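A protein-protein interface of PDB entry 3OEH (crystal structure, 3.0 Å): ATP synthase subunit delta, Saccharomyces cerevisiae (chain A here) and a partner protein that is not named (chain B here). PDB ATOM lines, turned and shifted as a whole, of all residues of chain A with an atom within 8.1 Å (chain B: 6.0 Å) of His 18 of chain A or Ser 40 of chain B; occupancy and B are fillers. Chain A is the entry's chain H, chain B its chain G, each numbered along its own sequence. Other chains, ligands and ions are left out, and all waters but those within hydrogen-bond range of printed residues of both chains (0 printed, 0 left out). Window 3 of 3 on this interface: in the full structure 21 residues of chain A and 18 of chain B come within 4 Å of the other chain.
Of the 12 printed residues of chain A, 7 touch a printed residue of chain B.
Printed residues of chain A that touch a printed residue of chain B: Ala 15, Leu 16, Pro 17, His 18, Glu 19, Thr 20 and Ala 87.
Hydrophobic or aromatic side chains of chain A that line the printed part of chain B: Ala 15 and Pro 17.
Of the 11 printed residues of chain B, 4 touch a printed residue of chain A.
Hydrophobic or aromatic side chains of chain B within 4 Å of the printed part of chain A: Met 44.
A ring nitrogen (NE2) of His 18 of chain A lies within hydrogen-bond range of the backbone carbonyl oxygen (O) of Ile 88 of chain A, at 2.8 Å.
O of Lys 36 of chain B sits close to OG of Ser 40 of chain B (3.4 Å).
The backbone carbonyl oxygen (O) of Ala 15 of chain A is in hydrogen-bond range of the backbone NH (N) of Ala 87 of chain A (3.1 Å).
OE1 of Glu 89 of chain A lies within hydrogen-bond range of NE2 of His 18 of chain A.
Of the printed residues of chain B, Ala 15 of chain A touches Met 44 (3.7 Å).
Of the printed residues of chain B, Thr 20 of chain A touches Ser 40 and Lys 43.
Glu 35 of chain B touches none of the printed residues of chain A.
Lys 36 of chain B touches none of the printed residues of chain A.
Ser 40 of chain B touches five residues of chain A.
Ala 41 of chain B touches just one residue of chain A: Pro 17.
Of the printed residues of chain A, Lys 43 of chain B touches Thr 20 (3.96 Å).
Of the printed residues of chain A, Met 44 of chain B touches Ala 15, Leu 16, Pro 17 and Ala 87.
The nearest residue of chain B that does not touch His 18 of chain A is Lys 36 of chain B (4.03 Å).
The nearest residue of chain A that does not touch Ser 40 of chain B is Ala 15 of chain A (5.6 Å).
The nearest printed residue of chain B that does not touch Ala 87 of chain A is Ser 40 of chain B (7.8 Å).
Met 44 of chain B touches Ala 15 of chain A (CE to O, 3.7 Å).
Met 44 of chain B touches Leu 16 of chain A.
O of Pro 17 of chain A touches CB of Ser 40 of chain B, 3.1 Å away.
O of Pro 17 of chain A touches N of Ala 41 of chain B, at 3.7 Å.
CE of Met 44 of chain B touches CD of Pro 17 of chain A, at 3.6 Å.
Glu 19 of chain A touches Ser 40 of chain B.
OG of Ser 40 of chain B touches CG2 of Thr 20 of chain A (3.4 Å).
Lys 43 of chain B touches Thr 20 of chain A.
Ala 87 of chain A touches Met 44 of chain B (O to CE, 3.5 Å).
O of His 18 of chain A is in hydrogen-bond range of OG of Ser 40 of chain B (2.6 Å).
O of Leu 16 of chain A lies close to O of Ser 40 of chain B (3.0 Å).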
ATOM      1  N   ALA A  15     -19.823  12.227  -8.188  1.00  0.00           N
ATOM      2  CA  ALA A  15     -20.591  11.564  -9.266  1.00  0.00           C
ATOM      3  C   ALA A  15     -21.996  12.117  -9.540  1.00  0.00           C
ATOM      4  O   ALA A  15     -22.753  12.411  -8.617  1.00  0.00           O
ATOM      5  CB  ALA A  15     -20.662  10.059  -9.027  1.00  0.00           C
ATOM      6  N   LEU A  16     -22.331  12.242 -10.824  1.00  0.00           N
ATOM      7  CA  LEU A  16     -23.683  12.606 -11.268  1.00  0.00           C
ATOM      8  C   LEU A  16     -24.249  11.484 -12.153  1.00  0.00           C
ATOM      9  O   LEU A  16     -23.473  10.703 -12.720  1.00  0.00           O
ATOM     10  CB  LEU A  16     -23.659  13.923 -12.053  1.00  0.00           C
ATOM     11  CG  LEU A  16     -22.730  15.051 -11.601  1.00  0.00           C
ATOM     12  CD1 LEU A  16     -22.396  15.959 -12.775  1.00  0.00           C
ATOM     13  CD2 LEU A  16     -23.339  15.842 -10.455  1.00  0.00           C
ATOM     14  N   PRO A  17     -25.596  11.399 -12.285  1.00  0.00           N
ATOM     15  CA  PRO A  17     -26.194  10.345 -13.112  1.00  0.00           C
ATOM     16  C   PRO A  17     -25.930  10.537 -14.604  1.00  0.00           C
ATOM     17  O   PRO A  17     -25.787   9.546 -15.319  1.00  0.00           O
ATOM     18  CB  PRO A  17     -27.690  10.466 -12.815  1.00  0.00           C
ATOM     19  CG  PRO A  17     -27.884  11.884 -12.434  1.00  0.00           C
ATOM     20  CD  PRO A  17     -26.628  12.295 -11.724  1.00  0.00           C
ATOM     21  N   HIS A  18     -25.868  11.789 -15.066  1.00  0.00           N
ATOM     22  CA  HIS A  18     -25.539  12.067 -16.466  1.00  0.00           C
ATOM     23  C   HIS A  18     -24.045  12.216 -16.737  1.00  0.00           C
ATOM     24  O   HIS A  18     -23.521  11.571 -17.639  1.00  0.00           O
ATOM     25  CB  HIS A  18     -26.349  13.242 -17.055  1.00  0.00           C
ATOM     26  CG  HIS A  18     -26.305  14.507 -16.249  1.00  0.00           C
ATOM     27  ND1 HIS A  18     -25.317  15.457 -16.404  1.00  0.00           N
ATOM     28  CD2 HIS A  18     -27.163  15.006 -15.326  1.00  0.00           C
ATOM     29  CE1 HIS A  18     -25.552  16.472 -15.592  1.00  0.00           C
ATOM     30  NE2 HIS A  18     -26.669  16.226 -14.931  1.00  0.00           N
ATOM     31  N   GLU A  19     -23.365  13.050 -15.957  1.00  0.00           N
ATOM     32  CA  GLU A  19     -21.911  13.232 -16.074  1.00  0.00           C
ATOM     33  C   GLU A  19     -21.191  12.672 -14.826  1.00  0.00           C
ATOM     34  O   GLU A  19     -21.816  12.480 -13.782  1.00  0.00           O
ATOM     35  CB  GLU A  19     -21.594  14.718 -16.331  1.00  0.00           C
ATOM     36  CG  GLU A  19     -20.182  15.211 -15.971  1.00  0.00           C
ATOM     37  CD  GLU A  19     -19.120  14.859 -17.007  1.00  0.00           C
ATOM     38  OE1 GLU A  19     -18.222  15.703 -17.244  1.00  0.00           O
ATOM     39  OE2 GLU A  19     -19.174  13.742 -17.573  1.00  0.00           O
ATOM     40  N   THR A  20     -19.894  12.384 -14.936  1.00  0.00           N
ATOM     41  CA  THR A  20     -19.123  11.868 -13.789  1.00  0.00           C
ATOM     42  C   THR A  20     -17.868  12.704 -13.490  1.00  0.00           C
ATOM     43  O   THR A  20     -16.842  12.571 -14.165  1.00  0.00           O
ATOM     44  CB  THR A  20     -18.795  10.356 -13.934  1.00  0.00           C
ATOM     45  OG1 THR A  20     -17.586  10.055 -13.224  1.00  0.00           O
ATOM     46  CG2 THR A  20     -18.638   9.960 -15.406  1.00  0.00           C
ATOM     47  N   LEU A  21     -17.947  13.536 -12.454  1.00  0.00           N
ATOM     48  CA  LEU A  21     -16.994  14.635 -12.275  1.00  0.00           C
ATOM     49  C   LEU A  21     -15.602  14.319 -11.729  1.00  0.00           C
ATOM     50  O   LEU A  21     -14.624  14.832 -12.263  1.00  0.00           O
ATOM     51  CB  LEU A  21     -17.619  15.774 -11.464  1.00  0.00           C
ATOM     52  CG  LEU A  21     -18.750  16.572 -12.116  1.00  0.00           C
ATOM     53  CD1 LEU A  21     -19.327  17.549 -11.118  1.00  0.00           C
ATOM     54  CD2 LEU A  21     -18.291  17.306 -13.372  1.00  0.00           C
ATOM     55  N   SER A  71     -27.539  20.515  -7.666  1.00  0.00           N
ATOM     56  CA  SER A  71     -28.962  20.289  -7.464  1.00  0.00           C
ATOM     57  C   SER A  71     -29.217  19.816  -6.039  1.00  0.00           C
ATOM     58  O   SER A  71     -30.139  20.284  -5.364  1.00  0.00           O
ATOM     59  CB  SER A  71     -29.464  19.233  -8.452  1.00  0.00           C
ATOM     60  OG  SER A  71     -28.669  18.055  -8.394  1.00  0.00           O
ATOM     61  N   ALA A  87     -24.809  14.018  -6.871  1.00  0.00           N
ATOM     62  CA  ALA A  87     -25.779  15.052  -7.199  1.00  0.00           C
ATOM     63  C   ALA A  87     -26.405  14.700  -8.533  1.00  0.00           C
ATOM     64  O   ALA A  87     -25.836  13.919  -9.296  1.00  0.00           O
ATOM     65  CB  ALA A  87     -25.110  16.408  -7.267  1.00  0.00           C
ATOM     66  N   ILE A  88     -27.582  15.256  -8.799  1.00  0.00           N
ATOM     67  CA  ILE A  88     -28.243  15.072 -10.087  1.00  0.00           C
ATOM     68  C   ILE A  88     -27.586  15.990 -11.111  1.00  0.00           C
ATOM     69  O   ILE A  88     -27.271  15.569 -12.226  1.00  0.00           O
ATOM     70  CB  ILE A  88     -29.748  15.404 -10.017  1.00  0.00           C
ATOM     71  CG1 ILE A  88     -30.389  14.768  -8.780  1.00  0.00           C
ATOM     72  CG2 ILE A  88     -30.457  14.981 -11.309  1.00  0.00           C
ATOM     73  CD1 ILE A  88     -31.433  15.651  -8.143  1.00  0.00           C
ATOM     74  N   GLU A  89     -27.372  17.240 -10.702  1.00  0.00           N
ATOM     75  CA  GLU A  89     -26.893  18.300 -11.581  1.00  0.00           C
ATOM     76  C   GLU A  89     -25.633  18.956 -11.029  1.00  0.00           C
ATOM     77  O   GLU A  89     -25.511  19.152  -9.819  1.00  0.00           O
ATOM     78  CB  GLU A  89     -27.975  19.378 -11.751  1.00  0.00           C
ATOM     79  CG  GLU A  89     -29.279  18.918 -12.395  1.00  0.00           C
ATOM     80  CD  GLU A  89     -29.299  19.146 -13.889  1.00  0.00           C
ATOM     81  OE1 GLU A  89     -28.384  18.640 -14.577  1.00  0.00           O
ATOM     82  OE2 GLU A  89     -30.231  19.832 -14.375  1.00  0.00           O
ATOM     83  N   ALA A  90     -24.713  19.306 -11.928  1.00  0.00           N
ATOM     84  CA  ALA A  90     -23.542  20.121 -11.590  1.00  0.00           C
ATOM     85  C   ALA A  90     -23.553  21.448 -12.350  1.00  0.00           C
ATOM     86  O   ALA A  90     -24.610  22.045 -12.576  1.00  0.00           O
ATOM     87  CB  ALA A  90     -22.266  19.367 -11.880  1.00  0.00           C
ATOM     88  N   GLU B  35     -23.926   4.593 -23.832  1.00  0.00           N
ATOM     89  CA  GLU B  35     -22.789   3.996 -23.132  1.00  0.00           C
ATOM     90  C   GLU B  35     -22.238   5.011 -22.135  1.00  0.00           C
ATOM     91  O   GLU B  35     -21.778   4.649 -21.049  1.00  0.00           O
ATOM     92  CB  GLU B  35     -21.697   3.578 -24.120  1.00  0.00           C
ATOM     93  CG  GLU B  35     -21.887   2.186 -24.714  1.00  0.00           C
ATOM     94  CD  GLU B  35     -21.198   1.090 -23.909  1.00  0.00           C
ATOM     95  OE1 GLU B  35     -20.477   0.278 -24.527  1.00  0.00           O
ATOM     96  OE2 GLU B  35     -21.369   1.038 -22.670  1.00  0.00           O
ATOM     97  N   LYS B  36     -22.301   6.283 -22.530  1.00  0.00           N
ATOM     98  CA  LYS B  36     -21.922   7.413 -21.686  1.00  0.00           C
ATOM     99  C   LYS B  36     -22.970   7.673 -20.598  1.00  0.00           C
ATOM    100  O   LYS B  36     -22.627   8.103 -19.497  1.00  0.00           O
ATOM    101  CB  LYS B  36     -21.715   8.663 -22.547  1.00  0.00           C
ATOM    102  CG  LYS B  36     -20.795   9.715 -21.939  1.00  0.00           C
ATOM    103  CD  LYS B  36     -20.298  10.677 -23.015  1.00  0.00           C
ATOM    104  CE  LYS B  36     -19.147  11.537 -22.515  1.00  0.00           C
ATOM    105  NZ  LYS B  36     -18.488  12.262 -23.637  1.00  0.00           N
ATOM    106  N   ALA B  37     -24.240   7.421 -20.919  1.00  0.00           N
ATOM    107  CA  ALA B  37     -25.336   7.521 -19.951  1.00  0.00           C
ATOM    108  C   ALA B  37     -25.351   6.305 -19.027  1.00  0.00           C
ATOM    109  O   ALA B  37     -25.870   6.368 -17.903  1.00  0.00           O
ATOM    110  CB  ALA B  37     -26.675   7.665 -20.665  1.00  0.00           C
ATOM    111  N   LYS B  38     -24.780   5.200 -19.508  1.00  0.00           N
ATOM    112  CA  LYS B  38     -24.648   3.984 -18.711  1.00  0.00           C
ATOM    113  C   LYS B  38     -23.507   4.112 -17.708  1.00  0.00           C
ATOM    114  O   LYS B  38     -23.710   3.875 -16.521  1.00  0.00           O
ATOM    115  CB  LYS B  38     -24.433   2.760 -19.604  1.00  0.00           C
ATOM    116  CG  LYS B  38     -24.496   1.429 -18.857  1.00  0.00           C
ATOM    117  CD  LYS B  38     -23.992   0.273 -19.713  1.00  0.00           C
ATOM    118  CE  LYS B  38     -22.482   0.097 -19.609  1.00  0.00           C
ATOM    119  NZ  LYS B  38     -22.031  -1.132 -20.322  1.00  0.00           N
ATOM    120  N   ILE B  39     -22.319   4.481 -18.197  1.00  0.00           N
ATOM    121  CA  ILE B  39     -21.121   4.649 -17.362  1.00  0.00           C
ATOM    122  C   ILE B  39     -21.350   5.643 -16.223  1.00  0.00           C
ATOM    123  O   ILE B  39     -20.960   5.386 -15.079  1.00  0.00           O
ATOM    124  CB  ILE B  39     -19.879   5.074 -18.206  1.00  0.00           C
ATOM    125  CG1 ILE B  39     -19.320   3.884 -19.005  1.00  0.00           C
ATOM    126  CG2 ILE B  39     -18.791   5.720 -17.328  1.00  0.00           C
ATOM    127  CD1 ILE B  39     -18.799   2.712 -18.159  1.00  0.00           C
ATOM    128  N   SER B  40     -21.997   6.762 -16.547  1.00  0.00           N
ATOM    129  CA  SER B  40     -22.326   7.789 -15.565  1.00  0.00           C
ATOM    130  C   SER B  40     -23.330   7.296 -14.531  1.00  0.00           C
ATOM    131  O   SER B  40     -23.383   7.819 -13.417  1.00  0.00           O
ATOM    132  CB  SER B  40     -22.843   9.047 -16.254  1.00  0.00           C
ATOM    133  OG  SER B  40     -21.772   9.873 -16.668  1.00  0.00           O
ATOM    134  N   ALA B  41     -24.119   6.291 -14.905  1.00  0.00           N
ATOM    135  CA  ALA B  41     -25.003   5.605 -13.961  1.00  0.00           C
ATOM    136  C   ALA B  41     -24.259   4.552 -13.126  1.00  0.00           C
ATOM    137  O   ALA B  41     -24.468   4.469 -11.914  1.00  0.00           O
ATOM    138  CB  ALA B  41     -26.179   4.975 -14.689  1.00  0.00           C
ATOM    139  N   LYS B  42     -23.389   3.766 -13.767  1.00  0.00           N
ATOM    140  CA  LYS B  42     -22.688   2.663 -13.096  1.00  0.00           C
ATOM    141  C   LYS B  42     -21.589   3.151 -12.160  1.00  0.00           C
ATOM    142  O   LYS B  42     -21.399   2.590 -11.081  1.00  0.00           O
ATOM    143  CB  LYS B  42     -22.110   1.681 -14.109  1.00  0.00           C
ATOM    144  CG  LYS B  42     -22.177   0.218 -13.672  1.00  0.00           C
ATOM    145  CD  LYS B  42     -21.835  -0.702 -14.848  1.00  0.00           C
ATOM    146  CE  LYS B  42     -22.660  -1.985 -14.843  1.00  0.00           C
ATOM    147  NZ  LYS B  42     -22.804  -2.548 -16.222  1.00  0.00           N
ATOM    148  N   LYS B  43     -20.866   4.187 -12.585  1.00  0.00           N
ATOM    149  CA  LYS B  43     -19.870   4.852 -11.740  1.00  0.00           C
ATOM    150  C   LYS B  43     -20.529   5.420 -10.485  1.00  0.00           C
ATOM    151  O   LYS B  43     -19.961   5.352  -9.397  1.00  0.00           O
ATOM    152  CB  LYS B  43     -19.179   5.981 -12.511  1.00  0.00           C
ATOM    153  CG  LYS B  43     -17.748   6.260 -12.087  1.00  0.00           C
ATOM    154  CD  LYS B  43     -16.766   5.333 -12.803  1.00  0.00           C
ATOM    155  CE  LYS B  43     -15.358   5.453 -12.240  1.00  0.00           C
ATOM    156  NZ  LYS B  43     -15.282   4.998 -10.818  1.00  0.00           N
ATOM    157  N   MET B  44     -21.732   5.964 -10.648  1.00  0.00           N
ATOM    158  CA  MET B  44     -22.472   6.569  -9.547  1.00  0.00           C
ATOM    159  C   MET B  44     -23.047   5.534  -8.581  1.00  0.00           C
ATOM    160  O   MET B  44     -23.421   5.874  -7.452  1.00  0.00           O
ATOM    161  CB  MET B  44     -23.598   7.446 -10.079  1.00  0.00           C
ATOM    162  CG  MET B  44     -24.060   8.492  -9.101  1.00  0.00           C
ATOM    163  SD  MET B  44     -25.801   8.810  -9.327  1.00  0.00           S
ATOM    164  CE  MET B  44     -25.897  10.471  -8.669  1.00  0.00           C
ATOM    165  N   ASP B  45     -23.130   4.280  -9.021  1.00  0.00           N
ATOM    166  CA  ASP B  45     -23.615   3.226  -8.139  1.00  0.00           C
ATOM    167  C   ASP B  45     -22.592   2.870  -7.060  1.00  0.00           C
ATOM    168  O   ASP B  45     -22.935   2.795  -5.875  1.00  0.00           O
ATOM    169  CB  ASP B  45     -24.066   1.978  -8.906  1.00  0.00           C
ATOM    170  CG  ASP B  45     -25.059   1.137  -8.103  1.00  0.00           C
ATOM    171  OD1 ASP B  45     -26.132   1.681  -7.723  1.00  0.00           O
ATOM    172  OD2 ASP B  45     -24.760  -0.054  -7.837  1.00  0.00           O
